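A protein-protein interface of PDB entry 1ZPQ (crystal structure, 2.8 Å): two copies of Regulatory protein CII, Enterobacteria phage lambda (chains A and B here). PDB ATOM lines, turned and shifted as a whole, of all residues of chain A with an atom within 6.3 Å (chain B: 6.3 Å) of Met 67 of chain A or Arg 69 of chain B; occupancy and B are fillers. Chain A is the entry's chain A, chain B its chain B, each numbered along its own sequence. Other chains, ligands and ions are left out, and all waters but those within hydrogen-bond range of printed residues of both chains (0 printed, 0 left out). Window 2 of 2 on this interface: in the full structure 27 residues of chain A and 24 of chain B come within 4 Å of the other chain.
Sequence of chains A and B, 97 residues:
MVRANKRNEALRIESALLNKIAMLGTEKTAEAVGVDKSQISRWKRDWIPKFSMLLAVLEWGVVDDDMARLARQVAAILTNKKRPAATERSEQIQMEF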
ATOM      1  N   GLY A  61     -20.586  -8.244  -9.841  1.00  0.00           N
ATOM      2  CA  GLY A  61     -19.156  -8.152 -10.318  1.00  0.00           C
ATOM      3  C   GLY A  61     -18.412  -6.800 -10.275  1.00  0.00           C
ATOM      4  O   GLY A  61     -17.212  -6.768 -10.031  1.00  0.00           O
ATOM      5  N   VAL A  62     -19.124  -5.699 -10.510  1.00  0.00           N
ATOM      6  CA  VAL A  62     -18.352  -4.430 -10.351  1.00  0.00           C
ATOM      7  C   VAL A  62     -16.948  -4.798 -10.754  1.00  0.00           C
ATOM      8  O   VAL A  62     -16.083  -4.859  -9.901  1.00  0.00           O
ATOM      9  CB  VAL A  62     -18.502  -3.173  -9.421  1.00  0.00           C
ATOM     10  CG1 VAL A  62     -17.602  -2.043  -9.773  1.00  0.00           C
ATOM     11  CG2 VAL A  62     -19.915  -2.649  -9.563  1.00  0.00           C
ATOM     12  N   VAL A  63     -16.785  -5.135 -12.010  1.00  0.00           N
ATOM     13  CA  VAL A  63     -15.570  -5.737 -12.526  1.00  0.00           C
ATOM     14  C   VAL A  63     -14.345  -4.879 -12.536  1.00  0.00           C
ATOM     15  O   VAL A  63     -14.419  -3.638 -12.582  1.00  0.00           O
ATOM     16  CB  VAL A  63     -15.774  -6.155 -14.000  1.00  0.00           C
ATOM     17  CG1 VAL A  63     -14.680  -7.106 -14.443  1.00  0.00           C
ATOM     18  CG2 VAL A  63     -17.140  -6.800 -14.195  1.00  0.00           C
ATOM     19  N   ASP A  64     -13.214  -5.577 -12.483  1.00  0.00           N
ATOM     20  CA  ASP A  64     -11.947  -4.863 -12.915  1.00  0.00           C
ATOM     21  C   ASP A  64     -12.014  -3.420 -13.438  1.00  0.00           C
ATOM     22  O   ASP A  64     -11.558  -2.496 -12.740  1.00  0.00           O
ATOM     23  CB  ASP A  64     -10.983  -5.708 -13.781  1.00  0.00           C
ATOM     24  CG  ASP A  64     -10.357  -6.897 -12.999  1.00  0.00           C
ATOM     25  OD1 ASP A  64     -11.149  -7.774 -12.560  1.00  0.00           O
ATOM     26  OD2 ASP A  64      -9.101  -7.032 -12.796  1.00  0.00           O
ATOM     27  N   ASP A  65     -12.544  -3.210 -14.639  1.00  0.00           N
ATOM     28  CA  ASP A  65     -12.399  -1.889 -15.199  1.00  0.00           C
ATOM     29  C   ASP A  65     -13.217  -0.898 -14.403  1.00  0.00           C
ATOM     30  O   ASP A  65     -12.878   0.297 -14.299  1.00  0.00           O
ATOM     31  CB  ASP A  65     -12.796  -1.837 -16.653  1.00  0.00           C
ATOM     32  CG  ASP A  65     -12.441  -0.487 -17.288  1.00  0.00           C
ATOM     33  OD1 ASP A  65     -12.321  -0.466 -18.533  1.00  0.00           O
ATOM     34  OD2 ASP A  65     -12.246   0.591 -16.629  1.00  0.00           O
ATOM     35  N   ASP A  66     -14.304  -1.409 -13.850  1.00  0.00           N
ATOM     36  CA  ASP A  66     -15.144  -0.677 -12.907  1.00  0.00           C
ATOM     37  C   ASP A  66     -14.348  -0.330 -11.670  1.00  0.00           C
ATOM     38  O   ASP A  66     -14.343   0.784 -11.229  1.00  0.00           O
ATOM     39  CB  ASP A  66     -16.297  -1.556 -12.498  1.00  0.00           C
ATOM     40  CG  ASP A  66     -17.548  -1.232 -13.218  1.00  0.00           C
ATOM     41  OD1 ASP A  66     -18.519  -1.996 -13.010  1.00  0.00           O
ATOM     42  OD2 ASP A  66     -17.661  -0.254 -13.988  1.00  0.00           O
ATOM     43  N   MET A  67     -13.644  -1.318 -11.154  1.00  0.00           N
ATOM     44  CA  MET A  67     -12.736  -1.160 -10.064  1.00  0.00           C
ATOM     45  C   MET A  67     -11.549  -0.263 -10.403  1.00  0.00           C
ATOM     46  O   MET A  67     -10.866   0.228  -9.515  1.00  0.00           O
ATOM     47  CB  MET A  67     -12.230  -2.524  -9.697  1.00  0.00           C
ATOM     48  CG  MET A  67     -11.625  -2.590  -8.329  1.00  0.00           C
ATOM     49  SD  MET A  67     -12.697  -3.453  -7.194  1.00  0.00           S
ATOM     50  CE  MET A  67     -13.863  -2.052  -6.536  1.00  0.00           C
ATOM     51  N   ALA A  68     -11.288  -0.050 -11.686  1.00  0.00           N
ATOM     52  CA  ALA A  68     -10.170   0.763 -12.102  1.00  0.00           C
ATOM     53  C   ALA A  68     -10.592   2.207 -12.135  1.00  0.00           C
ATOM     54  O   ALA A  68     -10.006   2.997 -11.427  1.00  0.00           O
ATOM     55  CB  ALA A  68      -9.683   0.330 -13.395  1.00  0.00           C
ATOM     56  N   ARG A  69     -11.612   2.576 -12.903  1.00  0.00           N
ATOM     57  CA  ARG A  69     -12.089   3.977 -12.849  1.00  0.00           C
ATOM     58  C   ARG A  69     -12.353   4.530 -11.400  1.00  0.00           C
ATOM     59  O   ARG A  69     -12.132   5.724 -11.125  1.00  0.00           O
ATOM     60  CB  ARG A  69     -13.284   4.211 -13.784  1.00  0.00           C
ATOM     61  CG  ARG A  69     -14.445   3.309 -13.534  1.00  0.00           C
ATOM     62  CD  ARG A  69     -15.860   3.872 -13.933  1.00  0.00           C
ATOM     63  NE  ARG A  69     -16.683   4.350 -12.787  1.00  0.00           N
ATOM     64  CZ  ARG A  69     -17.991   4.707 -12.853  1.00  0.00           C
ATOM     65  NH1 ARG A  69     -18.695   4.615 -14.003  1.00  0.00           N
ATOM     66  NH2 ARG A  69     -18.614   5.137 -11.753  1.00  0.00           N
ATOM     67  N   LEU A  70     -12.798   3.664 -10.478  1.00  0.00           N
ATOM     68  CA  LEU A  70     -12.963   4.030  -9.084  1.00  0.00           C
ATOM     69  C   LEU A  70     -11.620   4.295  -8.532  1.00  0.00           C
ATOM     70  O   LEU A  70     -11.306   5.437  -8.245  1.00  0.00           O
ATOM     71  CB  LEU A  70     -13.563   2.913  -8.269  1.00  0.00           C
ATOM     72  CG  LEU A  70     -14.986   2.612  -8.558  1.00  0.00           C
ATOM     73  CD1 LEU A  70     -15.372   1.375  -7.757  1.00  0.00           C
ATOM     74  CD2 LEU A  70     -15.892   3.753  -8.217  1.00  0.00           C
ATOM     75  N   ALA A  71     -10.822   3.231  -8.432  1.00  0.00           N
ATOM     76  CA  ALA A  71      -9.484   3.274  -7.840  1.00  0.00           C
ATOM     77  C   ALA A  71      -8.659   4.410  -8.388  1.00  0.00           C
ATOM     78  O   ALA A  71      -7.804   4.930  -7.688  1.00  0.00           O
ATOM     79  CB  ALA A  71      -8.765   1.987  -8.065  1.00  0.00           C
ATOM     80  N   ARG A  72      -8.928   4.794  -9.636  1.00  0.00           N
ATOM     81  CA  ARG A  72      -8.271   5.920 -10.291  1.00  0.00           C
ATOM     82  C   ARG A  72      -8.611   7.266  -9.650  1.00  0.00           C
ATOM     83  O   ARG A  72      -7.701   7.953  -9.132  1.00  0.00           O
ATOM     84  CB  ARG A  72      -8.690   5.997 -11.757  1.00  0.00           C
ATOM     85  CG  ARG A  72      -7.848   5.207 -12.731  1.00  0.00           C
ATOM     86  CD  ARG A  72      -8.307   5.458 -14.147  1.00  0.00           C
ATOM     87  NE  ARG A  72      -8.372   4.219 -14.924  1.00  0.00           N
ATOM     88  CZ  ARG A  72      -9.361   3.881 -15.758  1.00  0.00           C
ATOM     89  NH1 ARG A  72     -10.408   4.686 -15.932  1.00  0.00           N
ATOM     90  NH2 ARG A  72      -9.299   2.727 -16.440  1.00  0.00           N
ATOM     91  N   MET B  23     -19.289   2.316  -4.185  1.00  0.00           N
ATOM     92  CA  MET B  23     -18.451   1.715  -5.238  1.00  0.00           C
ATOM     93  C   MET B  23     -19.307   1.625  -6.439  1.00  0.00           C
ATOM     94  O   MET B  23     -19.116   2.264  -7.371  1.00  0.00           O
ATOM     95  CB  MET B  23     -17.820   0.372  -4.841  1.00  0.00           C
ATOM     96  CG  MET B  23     -16.455   0.571  -4.283  1.00  0.00           C
ATOM     97  SD  MET B  23     -15.740  -0.952  -3.903  1.00  0.00           S
ATOM     98  CE  MET B  23     -16.725  -1.474  -2.443  1.00  0.00           C
ATOM     99  N   ASP B  65     -14.529  -6.934   1.145  1.00  0.00           N
ATOM    100  CA  ASP B  65     -13.370  -7.476   0.479  1.00  0.00           C
ATOM    101  C   ASP B  65     -13.055  -6.513  -0.622  1.00  0.00           C
ATOM    102  O   ASP B  65     -11.885  -6.279  -0.916  1.00  0.00           O
ATOM    103  CB  ASP B  65     -13.664  -8.872  -0.106  1.00  0.00           C
ATOM    104  CG  ASP B  65     -13.567  -9.988   0.939  1.00  0.00           C
ATOM    105  OD1 ASP B  65     -12.729  -9.893   1.861  1.00  0.00           O
ATOM    106  OD2 ASP B  65     -14.311 -10.987   0.937  1.00  0.00           O
ATOM    107  N   ASP B  66     -14.117  -5.980  -1.234  1.00  0.00           N
ATOM    108  CA  ASP B  66     -14.023  -5.117  -2.401  1.00  0.00           C
ATOM    109  C   ASP B  66     -13.414  -3.788  -1.957  1.00  0.00           C
ATOM    110  O   ASP B  66     -12.656  -3.174  -2.709  1.00  0.00           O
ATOM    111  CB  ASP B  66     -15.426  -4.882  -3.048  1.00  0.00           C
ATOM    112  CG  ASP B  66     -15.640  -5.600  -4.421  1.00  0.00           C
ATOM    113  OD1 ASP B  66     -14.691  -6.127  -5.042  1.00  0.00           O
ATOM    114  OD2 ASP B  66     -16.770  -5.643  -4.946  1.00  0.00           O
ATOM    115  N   MET B  67     -13.754  -3.342  -0.746  1.00  0.00           N
ATOM    116  CA  MET B  67     -13.255  -2.054  -0.244  1.00  0.00           C
ATOM    117  C   MET B  67     -11.802  -2.224   0.188  1.00  0.00           C
ATOM    118  O   MET B  67     -11.076  -1.263   0.398  1.00  0.00           O
ATOM    119  CB  MET B  67     -14.139  -1.511   0.885  1.00  0.00           C
ATOM    120  CG  MET B  67     -13.624  -0.242   1.575  1.00  0.00           C
ATOM    121  SD  MET B  67     -13.938   1.367   0.822  1.00  0.00           S
ATOM    122  CE  MET B  67     -12.540   1.512  -0.068  1.00  0.00           C
ATOM    123  N   ALA B  68     -11.398  -3.506   0.185  1.00  0.00           N
ATOM    124  CA  ALA B  68     -10.043  -3.791   0.332  1.00  0.00           C
ATOM    125  C   ALA B  68      -9.376  -3.490  -1.037  1.00  0.00           C
ATOM    126  O   ALA B  68      -8.338  -2.846  -1.115  1.00  0.00           O
ATOM    127  CB  ALA B  68      -9.808  -5.230   0.728  1.00  0.00           C
ATOM    128  N   ARG B  69      -9.999  -3.989  -2.104  1.00  0.00           N
ATOM    129  CA  ARG B  69      -9.202  -4.110  -3.411  1.00  0.00           C
ATOM    130  C   ARG B  69      -8.920  -2.676  -3.757  1.00  0.00           C
ATOM    131  O   ARG B  69      -7.925  -2.408  -4.398  1.00  0.00           O
ATOM    132  CB  ARG B  69     -10.117  -4.695  -4.512  1.00  0.00           C
ATOM    133  CG  ARG B  69     -11.026  -5.847  -4.089  1.00  0.00           C
ATOM    134  CD  ARG B  69     -10.357  -7.188  -4.050  1.00  0.00           C
ATOM    135  NE  ARG B  69     -11.289  -8.272  -3.707  1.00  0.00           N
ATOM    136  CZ  ARG B  69     -11.049  -9.584  -3.897  1.00  0.00           C
ATOM    137  NH1 ARG B  69      -9.906 -10.012  -4.428  1.00  0.00           N
ATOM    138  NH2 ARG B  69     -11.956 -10.482  -3.544  1.00  0.00           N
ATOM    139  N   LEU B  70      -9.806  -1.772  -3.348  1.00  0.00           N
ATOM    140  CA  LEU B  70      -9.673  -0.351  -3.640  1.00  0.00           C
ATOM    141  C   LEU B  70      -8.604   0.284  -2.814  1.00  0.00           C
ATOM    142  O   LEU B  70      -7.696   0.855  -3.340  1.00  0.00           O
ATOM    143  CB  LEU B  70     -10.965   0.370  -3.336  1.00  0.00           C
ATOM    144  CG  LEU B  70     -11.745   0.959  -4.476  1.00  0.00           C
ATOM    145  CD1 LEU B  70     -12.911   1.634  -3.826  1.00  0.00           C
ATOM    146  CD2 LEU B  70     -10.967   1.945  -5.258  1.00  0.00           C
ATOM    147  N   ALA B  71      -8.739   0.213  -1.507  1.00  0.00           N
ATOM    148  CA  ALA B  71      -7.699   0.680  -0.621  1.00  0.00           C
ATOM    149  C   ALA B  71      -6.340   0.282  -1.166  1.00  0.00           C
ATOM    150  O   ALA B  71      -5.438   1.103  -1.319  1.00  0.00           O
ATOM    151  CB  ALA B  71      -7.899   0.097   0.726  1.00  0.00           C
ATOM    152  N   ARG B  72      -6.184  -0.984  -1.484  1.00  0.00           N
ATOM    153  CA  ARG B  72      -4.914  -1.387  -2.014  1.00  0.00           C
ATOM    154  C   ARG B  72      -4.759  -0.962  -3.465  1.00  0.00           C
ATOM    155  O   ARG B  72      -3.696  -0.513  -3.823  1.00  0.00           O
ATOM    156  CB  ARG B  72      -4.677  -2.873  -1.827  1.00  0.00           C
ATOM    157  CG  ARG B  72      -5.554  -3.737  -2.630  1.00  0.00           C
ATOM    158  CD  ARG B  72      -5.806  -5.055  -1.949  1.00  0.00           C
ATOM    159  NE  ARG B  72      -6.399  -6.020  -2.877  1.00  0.00           N
ATOM    160  CZ  ARG B  72      -6.913  -7.194  -2.529  1.00  0.00           C
ATOM    161  NH1 ARG B  72      -6.936  -7.586  -1.255  1.00  0.00           N
ATOM    162  NH2 ARG B  72      -7.416  -7.980  -3.466  1.00  0.00           N
ATOM    163  N   GLN B  73      -5.790  -1.044  -4.291  1.00  0.00           N
ATOM    164  CA  GLN B  73      -5.657  -0.633  -5.690  1.00  0.00           C
ATOM    165  C   GLN B  73      -5.442   0.851  -5.863  1.00  0.00           C
ATOM    166  O   GLN B  73      -5.032   1.269  -6.929  1.00  0.00           O
ATOM    167  CB  GLN B  73      -6.883  -0.978  -6.522  1.00  0.00           C
ATOM    168  CG  GLN B  73      -6.731  -2.217  -7.367  1.00  0.00           C
ATOM    169  CD  GLN B  73      -7.930  -2.438  -8.260  1.00  0.00           C
ATOM    170  OE1 GLN B  73      -8.263  -1.533  -9.063  1.00  0.00           O
ATOM    171  NE2 GLN B  73      -8.541  -3.517  -8.152  1.00  0.00           N
ATOM    172  N   VAL B  74      -5.772   1.664  -4.870  1.00  0.00           N
ATOM    173  CA  VAL B  74      -5.381   3.059  -4.909  1.00  0.00           C
ATOM    174  C   VAL B  74      -3.921   3.071  -4.466  1.00  0.00           C
ATOM    175  O   VAL B  74      -3.163   3.915  -4.905  1.00  0.00           O
ATOM    176  CB  VAL B  74      -6.272   3.938  -4.043  1.00  0.00           C
ATOM    177  CG1 VAL B  74      -5.573   5.169  -3.629  1.00  0.00           C
ATOM    178  CG2 VAL B  74      -7.503   4.305  -4.789  1.00  0.00           C
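The guanidinium group (NE) of Arg 69 of chain B sits close to the backbone carbonyl oxygen (O) of Asp 65 of chain B (3.5 Å).
Of the 12 printed residues of chain A, 3 touch a printed residue of chain B.
Of the 11 printed residues of chain B, 6 touch a printed residue of chain A.
Hydrophobic or aromatic side chains of chain B within 4 Å of the printed part of chain A: Met 23, Leu 70 and Val 74.
Along chain B the printed residues that touch a printed residue of chain A span positions 23 to 74.
Among the printed residues, no Asp or Glu carboxylate lies within 4 Å of a Lys or Arg side-chain nitrogen of the other chain.
Among the printed residues, merely in contact across the chains: Ala 71 of chain A with Val 74 of chain B, Ala 71 of chain A with Leu 70 of chain B, Met 67 of chain A with Met 23 of chain B, Leu 70 of chain A with Met 23 of chain B, Ala 71 of chain A with Gln 73 of chain B, Met 67 of chain A with Arg 69 of chain B and Met 67 of chain A with Asp 66 of chain B.
O of Met 67 of chain A lies close to OE1 of Gln 73 of chain B (3.2 Å).
Of chain B, only Met 23, Asp 66, Arg 69 and Gln 73 come within 4 Å of Met 67 of chain A.
Of the printed residues of chain A, Met 23 of chain B touches Met 67 and Leu 70.
Of chain A, only Met 67 comes within 4 Å of Arg 69 of chain B.
Of the printed residues of chain A, Gln 73 of chain B touches Met 67 (3.2 Å) and Ala 71 (3.7 Å).
The nearest residue of chain B that does not touch Met 67 of chain A is Leu 70 of chain B (4.2 Å).
The nearest residue of chain A that does not touch Arg 69 of chain B is Ala 71 of chain A (5.8 Å).
Met 67 of chain A touches Asp 66 of chain B, but with the chains exchanged Asp 66 of chain A does not touch Met 67 of chain B (11.3 Å).
Met 67 of chain A touches Arg 69 of chain B, but with the chains exchanged Arg 69 of chain A does not touch Met 67 of chain B (11.7 Å).
Ala 71 of chain A touches Leu 70 of chain B, but with the chains exchanged Leu 70 of chain A does not touch Ala 71 of chain B (8.6 Å).
8 positions are printed for both chains.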
